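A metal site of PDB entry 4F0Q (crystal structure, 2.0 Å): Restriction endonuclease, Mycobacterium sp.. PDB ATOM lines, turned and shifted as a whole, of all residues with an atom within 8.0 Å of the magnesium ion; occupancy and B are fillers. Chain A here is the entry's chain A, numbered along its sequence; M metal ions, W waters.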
ATOM      1  N   LYS A 297     -18.574 -25.356 -19.267  1.00  0.00           N
ATOM      2  CA  LYS A 297     -19.717 -25.484 -18.377  1.00  0.00           C
ATOM      3  C   LYS A 297     -20.214 -24.143 -17.825  1.00  0.00           C
ATOM      4  O   LYS A 297     -21.388 -23.793 -17.974  1.00  0.00           O
ATOM      5  CB  LYS A 297     -19.358 -26.423 -17.221  1.00  0.00           C
ATOM      6  CG  LYS A 297     -20.447 -26.619 -16.184  1.00  0.00           C
ATOM      7  CD  LYS A 297     -19.959 -27.511 -15.045  1.00  0.00           C
ATOM      8  CE  LYS A 297     -21.024 -27.678 -13.982  1.00  0.00           C
ATOM      9  NZ  LYS A 297     -22.233 -28.377 -14.504  1.00  0.00           N
ATOM     10  N   HIS A 298     -19.321 -23.406 -17.185  1.00  0.00           N
ATOM     11  CA  HIS A 298     -19.704 -22.180 -16.483  1.00  0.00           C
ATOM     12  C   HIS A 298     -19.943 -20.999 -17.423  1.00  0.00           C
ATOM     13  O   HIS A 298     -20.697 -20.080 -17.100  1.00  0.00           O
ATOM     14  CB  HIS A 298     -18.670 -21.852 -15.414  1.00  0.00           C
ATOM     15  CG  HIS A 298     -18.417 -22.976 -14.448  1.00  0.00           C
ATOM     16  ND1 HIS A 298     -19.189 -23.187 -13.329  1.00  0.00           N
ATOM     17  CD2 HIS A 298     -17.502 -23.976 -14.468  1.00  0.00           C
ATOM     18  CE1 HIS A 298     -18.746 -24.252 -12.683  1.00  0.00           C
ATOM     19  NE2 HIS A 298     -17.724 -24.755 -13.357  1.00  0.00           N
ATOM     20  N   PHE A 300     -21.374 -21.535 -20.211  1.00  0.00           N
ATOM     21  CA  PHE A 300     -22.743 -21.900 -20.552  1.00  0.00           C
ATOM     22  C   PHE A 300     -23.686 -21.514 -19.425  1.00  0.00           C
ATOM     23  O   PHE A 300     -24.857 -21.243 -19.668  1.00  0.00           O
ATOM     24  CB  PHE A 300     -22.861 -23.396 -20.855  1.00  0.00           C
ATOM     25  CG  PHE A 300     -24.248 -23.823 -21.247  1.00  0.00           C
ATOM     26  CD1 PHE A 300     -24.743 -23.570 -22.511  1.00  0.00           C
ATOM     27  CD2 PHE A 300     -25.063 -24.474 -20.337  1.00  0.00           C
ATOM     28  CE1 PHE A 300     -26.016 -23.967 -22.870  1.00  0.00           C
ATOM     29  CE2 PHE A 300     -26.341 -24.870 -20.682  1.00  0.00           C
ATOM     30  CZ  PHE A 300     -26.822 -24.615 -21.950  1.00  0.00           C
ATOM     31  N   GLU A 301     -23.184 -21.503 -18.201  1.00  0.00           N
ATOM     32  CA  GLU A 301     -23.968 -21.029 -17.064  1.00  0.00           C
ATOM     33  C   GLU A 301     -24.265 -19.533 -17.180  1.00  0.00           C
ATOM     34  O   GLU A 301     -25.392 -19.096 -16.936  1.00  0.00           O
ATOM     35  CB  GLU A 301     -23.272 -21.349 -15.740  1.00  0.00           C
ATOM     36  CG  GLU A 301     -23.167 -22.835 -15.441  1.00  0.00           C
ATOM     37  CD  GLU A 301     -22.419 -23.115 -14.150  1.00  0.00           C
ATOM     38  OE1 GLU A 301     -21.800 -22.183 -13.602  1.00  0.00           O
ATOM     39  OE2 GLU A 301     -22.440 -24.282 -13.687  1.00  0.00           O
ATOM     40  N   ARG A 326     -20.426 -20.567  -8.984  1.00  0.00           N
ATOM     41  CA  ARG A 326     -18.995 -20.830  -8.936  1.00  0.00           C
ATOM     42  C   ARG A 326     -18.370 -20.782 -10.328  1.00  0.00           C
ATOM     43  O   ARG A 326     -19.069 -20.796 -11.339  1.00  0.00           O
ATOM     44  CB  ARG A 326     -18.706 -22.192  -8.294  1.00  0.00           C
ATOM     45  CG  ARG A 326     -19.421 -23.352  -8.954  1.00  0.00           C
ATOM     46  CD  ARG A 326     -20.685 -23.729  -8.196  1.00  0.00           C
ATOM     47  NE  ARG A 326     -21.693 -24.297  -9.076  1.00  0.00           N
ATOM     48  CZ  ARG A 326     -22.912 -24.654  -8.688  1.00  0.00           C
ATOM     49  NH1 ARG A 326     -23.274 -24.504  -7.417  1.00  0.00           N
ATOM     50  NH2 ARG A 326     -23.773 -25.159  -9.558  1.00  0.00           N
ATOM     51  N   GLY A 329     -16.239 -26.525 -10.626  1.00  0.00           N
ATOM     52  CA  GLY A 329     -16.996 -27.520  -9.876  1.00  0.00           C
ATOM     53  C   GLY A 329     -18.429 -27.616 -10.334  1.00  0.00           C
ATOM     54  O   GLY A 329     -18.772 -27.180 -11.440  1.00  0.00           O
ATOM     55  N   ASP A 330     -19.279 -28.184  -9.485  1.00  0.00           N
ATOM     56  CA  ASP A 330     -20.691 -28.372  -9.826  1.00  0.00           C
ATOM     57  C   ASP A 330     -21.571 -28.256  -8.583  1.00  0.00           C
ATOM     58  O   ASP A 330     -21.095 -28.379  -7.461  1.00  0.00           O
ATOM     59  CB  ASP A 330     -20.887 -29.745 -10.485  1.00  0.00           C
ATOM     60  CG  ASP A 330     -22.258 -29.904 -11.117  1.00  0.00           C
ATOM     61  OD1 ASP A 330     -22.838 -28.889 -11.545  1.00  0.00           O
ATOM     62  OD2 ASP A 330     -22.746 -31.049 -11.182  1.00  0.00           O
ATOM     63  N   GLY A 331     -22.850 -28.001  -8.798  1.00  0.00           N
ATOM     64  CA  GLY A 331     -23.812 -27.898  -7.714  1.00  0.00           C
ATOM     65  C   GLY A 331     -25.235 -27.906  -8.226  1.00  0.00           C
ATOM     66  O   GLY A 331     -25.470 -27.995  -9.428  1.00  0.00           O
ATOM     67  N   GLY A 332     -26.193 -27.804  -7.306  1.00  0.00           N
ATOM     68  CA  GLY A 332     -27.602 -27.810  -7.670  1.00  0.00           C
ATOM     69  C   GLY A 332     -28.020 -26.556  -8.422  1.00  0.00           C
ATOM     70  O   GLY A 332     -28.724 -26.637  -9.433  1.00  0.00           O
ATOM     71  N   VAL A 333     -27.593 -25.408  -7.921  1.00  0.00           N
ATOM     72  CA  VAL A 333     -27.941 -24.129  -8.526  1.00  0.00           C
ATOM     73  C   VAL A 333     -26.739 -23.521  -9.237  1.00  0.00           C
ATOM     74  O   VAL A 333     -25.638 -23.442  -8.675  1.00  0.00           O
ATOM     75  CB  VAL A 333     -28.459 -23.130  -7.471  1.00  0.00           C
ATOM     76  CG1 VAL A 333     -28.854 -21.816  -8.126  1.00  0.00           C
ATOM     77  CG2 VAL A 333     -29.630 -23.735  -6.720  1.00  0.00           C
ATOM     78  N   ASP A 334     -26.930 -23.094 -10.480  1.00  0.00           N
ATOM     79  CA  ASP A 334     -25.845 -22.560 -11.294  1.00  0.00           C
ATOM     80  C   ASP A 334     -25.803 -21.035 -11.304  1.00  0.00           C
ATOM     81  O   ASP A 334     -24.739 -20.446 -11.458  1.00  0.00           O
ATOM     82  CB  ASP A 334     -25.926 -23.102 -12.724  1.00  0.00           C
ATOM     83  CG  ASP A 334     -25.621 -24.586 -12.801  1.00  0.00           C
ATOM     84  OD1 ASP A 334     -25.743 -25.275 -11.768  1.00  0.00           O
ATOM     85  OD2 ASP A 334     -25.244 -25.062 -13.889  1.00  0.00           O
ATOM     86  N   PHE A 335     -26.961 -20.394 -11.150  1.00  0.00           N
ATOM     87  CA  PHE A 335     -27.013 -18.937 -11.077  1.00  0.00           C
ATOM     88  C   PHE A 335     -28.226 -18.410 -10.325  1.00  0.00           C
ATOM     89  O   PHE A 335     -29.226 -19.109 -10.158  1.00  0.00           O
ATOM     90  CB  PHE A 335     -26.905 -18.303 -12.467  1.00  0.00           C
ATOM     91  CG  PHE A 335     -28.001 -18.698 -13.413  1.00  0.00           C
ATOM     92  CD1 PHE A 335     -27.853 -19.806 -14.243  1.00  0.00           C
ATOM     93  CD2 PHE A 335     -29.172 -17.968 -13.492  1.00  0.00           C
ATOM     94  CE1 PHE A 335     -28.862 -20.174 -15.120  1.00  0.00           C
ATOM     95  CE2 PHE A 335     -30.181 -18.329 -14.362  1.00  0.00           C
ATOM     96  CZ  PHE A 335     -30.024 -19.433 -15.182  1.00  0.00           C
ATOM     97  N   GLY A 354     -31.319 -20.570 -10.887  1.00  0.00           N
ATOM     98  CA  GLY A 354     -31.038 -21.054 -12.215  1.00  0.00           C
ATOM     99  C   GLY A 354     -30.192 -22.300 -12.255  1.00  0.00           C
ATOM    100  O   GLY A 354     -29.339 -22.525 -11.394  1.00  0.00           O
ATOM    101  N   GLN A 355     -30.440 -23.140 -13.264  1.00  0.00           N
ATOM    102  CA  GLN A 355     -29.641 -24.337 -13.490  1.00  0.00           C
ATOM    103  C   GLN A 355     -29.392 -24.494 -14.984  1.00  0.00           C
ATOM    104  O   GLN A 355     -30.305 -24.367 -15.791  1.00  0.00           O
ATOM    105  CB  GLN A 355     -30.356 -25.572 -12.957  1.00  0.00           C
ATOM    106  CG  GLN A 355     -29.763 -26.883 -13.429  1.00  0.00           C
ATOM    107  CD  GLN A 355     -28.331 -27.070 -12.971  1.00  0.00           C
ATOM    108  OE1 GLN A 355     -27.460 -27.419 -13.774  1.00  0.00           O
ATOM    109  NE2 GLN A 355     -28.083 -26.849 -11.692  1.00  0.00           N
ATOM    110  N   ALA A 356     -28.149 -24.788 -15.352  1.00  0.00           N
ATOM    111  CA  ALA A 356     -27.774 -24.936 -16.747  1.00  0.00           C
ATOM    112  C   ALA A 356     -27.082 -26.265 -17.013  1.00  0.00           C
ATOM    113  O   ALA A 356     -26.159 -26.648 -16.296  1.00  0.00           O
ATOM    114  CB  ALA A 356     -26.879 -23.782 -17.173  1.00  0.00           C
ATOM    115  N   LYS A 357     -27.532 -26.976 -18.044  1.00  0.00           N
ATOM    116  CA  LYS A 357     -26.890 -28.232 -18.403  1.00  0.00           C
ATOM    117  C   LYS A 357     -26.773 -28.419 -19.914  1.00  0.00           C
ATOM    118  O   LYS A 357     -27.763 -28.581 -20.617  1.00  0.00           O
ATOM    119  CB  LYS A 357     -27.634 -29.424 -17.780  1.00  0.00           C
ATOM    120  CG  LYS A 357     -26.855 -30.727 -17.886  1.00  0.00           C
ATOM    121  CD  LYS A 357     -27.456 -31.809 -17.007  1.00  0.00           C
ATOM    122  CE  LYS A 357     -26.584 -33.059 -17.031  1.00  0.00           C
ATOM    123  NZ  LYS A 357     -27.107 -34.119 -16.122  1.00  0.00           N
ATOM    124  N   CYS A 358     -25.536 -28.390 -20.401  1.00  0.00           N
ATOM    125  CA  CYS A 358     -25.255 -28.538 -21.819  1.00  0.00           C
ATOM    126  C   CYS A 358     -25.043 -29.999 -22.200  1.00  0.00           C
ATOM    127  O   CYS A 358     -23.925 -30.502 -22.161  1.00  0.00           O
ATOM    128  CB  CYS A 358     -24.037 -27.706 -22.210  1.00  0.00           C
ATOM    129  SG  CYS A 358     -23.576 -27.828 -23.955  1.00  0.00           S
ATOM    130  N   ARG A 372     -33.693 -31.725  -8.458  1.00  0.00           N
ATOM    131  CA  ARG A 372     -32.538 -31.241  -7.692  1.00  0.00           C
ATOM    132  C   ARG A 372     -32.568 -29.731  -7.559  1.00  0.00           C
ATOM    133  O   ARG A 372     -32.039 -29.167  -6.594  1.00  0.00           O
ATOM    134  CB  ARG A 372     -31.221 -31.695  -8.337  1.00  0.00           C
ATOM    135  CG  ARG A 372     -30.017 -31.498  -7.435  1.00  0.00           C
ATOM    136  CD  ARG A 372     -28.738 -31.975  -8.096  1.00  0.00           C
ATOM    137  NE  ARG A 372     -27.595 -31.821  -7.200  1.00  0.00           N
ATOM    138  CZ  ARG A 372     -26.334 -32.039  -7.565  1.00  0.00           C
ATOM    139  NH1 ARG A 372     -26.049 -32.409  -8.809  1.00  0.00           N
ATOM    140  NH2 ARG A 372     -25.351 -31.873  -6.685  1.00  0.00           N
ATOM    141  N   VAL A 373     -33.178 -29.064  -8.526  1.00  0.00           N
ATOM    142  CA  VAL A 373     -33.307 -27.621  -8.506  1.00  0.00           C
ATOM    143  C   VAL A 373     -34.604 -27.213  -7.811  1.00  0.00           C
ATOM    144  O   VAL A 373     -34.644 -26.218  -7.088  1.00  0.00           O
ATOM    145  CB  VAL A 373     -33.287 -27.036  -9.926  1.00  0.00           C
ATOM    146  CG1 VAL A 373     -33.103 -25.530  -9.880  1.00  0.00           C
ATOM    147  CG2 VAL A 373     -32.190 -27.684 -10.744  1.00  0.00           C
ATOM    148  N   TYR A 385     -34.604 -23.827 -15.732  1.00  0.00           N
ATOM    149  CA  TYR A 385     -33.682 -24.846 -16.212  1.00  0.00           C
ATOM    150  C   TYR A 385     -33.380 -24.666 -17.696  1.00  0.00           C
ATOM    151  O   TYR A 385     -34.256 -24.852 -18.546  1.00  0.00           O
ATOM    152  CB  TYR A 385     -34.253 -26.247 -15.939  1.00  0.00           C
ATOM    153  CG  TYR A 385     -33.207 -27.323 -15.750  1.00  0.00           C
ATOM    154  CD1 TYR A 385     -32.154 -27.479 -16.647  1.00  0.00           C
ATOM    155  CD2 TYR A 385     -33.274 -28.195 -14.666  1.00  0.00           C
ATOM    156  CE1 TYR A 385     -31.200 -28.463 -16.477  1.00  0.00           C
ATOM    157  CE2 TYR A 385     -32.325 -29.185 -14.490  1.00  0.00           C
ATOM    158  CZ  TYR A 385     -31.292 -29.310 -15.390  1.00  0.00           C
ATOM    159  OH  TYR A 385     -30.344 -30.300 -15.214  1.00  0.00           O
ATOM    160  N   VAL A 386     -32.142 -24.293 -17.997  1.00  0.00           N
ATOM    161  CA  VAL A 386     -31.707 -24.076 -19.369  1.00  0.00           C
ATOM    162  C   VAL A 386     -30.840 -25.240 -19.862  1.00  0.00           C
ATOM    163  O   VAL A 386     -29.820 -25.586 -19.239  1.00  0.00           O
ATOM    164  CB  VAL A 386     -30.918 -22.771 -19.505  1.00  0.00           C
ATOM    165  CG1 VAL A 386     -30.496 -22.541 -20.950  1.00  0.00           C
ATOM    166  CG2 VAL A 386     -31.754 -21.605 -19.002  1.00  0.00           C
HETATM  167 MG    MG M   1     -25.484 -27.058 -14.375  1.00  0.00          MG
HETATM  168  O   HOH W   1     -23.777 -26.198 -15.211  1.00  0.00           O
HETATM  169  O   HOH W   2     -24.931 -27.341 -12.360  1.00  0.00           O
HETATM  170  O   HOH W   3     -24.898 -28.864 -15.240  1.00  0.00           O
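The magnesium ion is bound by the side-chain carboxylate (OD2) of Asp 334, 2.1 Å away. The backbone carbonyl oxygen (O) of Ala 356 is bound to the magnesium ion (2.1 Å). The magnesium ion is bound by water W1 (2.1 Å). Water W3 is bound to the magnesium ion, 2.1 Å away. The side-chain amide oxygen (OE1) of Gln 355 is bound to the magnesium ion (2.1 Å). Water W2 binds the magnesium ion (2.1 Å).
Lys 297 touches the magnesium ion. Four residues have an atom within 4 Å of the magnesium ion: Lys 297, Asp 334, Gln 355 and Ala 356.
Water W1 bridges the side-chain amino group (NZ) of Lys 297 and the side-chain carboxylate (OE2) of Glu 301. Water W2 lies within hydrogen-bond range of the side-chain carboxylate (OD1) of Asp 330 (2.7 Å), the backbone carbonyl oxygen (O) of Gly 331 (3.1 Å) and the side-chain amide nitrogen (NE2) of Gln 355 (3.3 Å).
OD1 of Asp 334 lies within salt-bridge range of NH2 of Arg 326 (3.0 Å). The backbone carbonyl oxygen (O) of Gly 354 lies within hydrogen-bond range of the backbone NH (N) of Asp 334. The backbone carbonyl oxygen of Gln 355 sits at hydrogen-bond distance from the backbone NH of Val 386, 2.9 Å away. OD1 of Asp 330 lies within salt-bridge range of NZ of Lys 297, at 3.1 Å.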
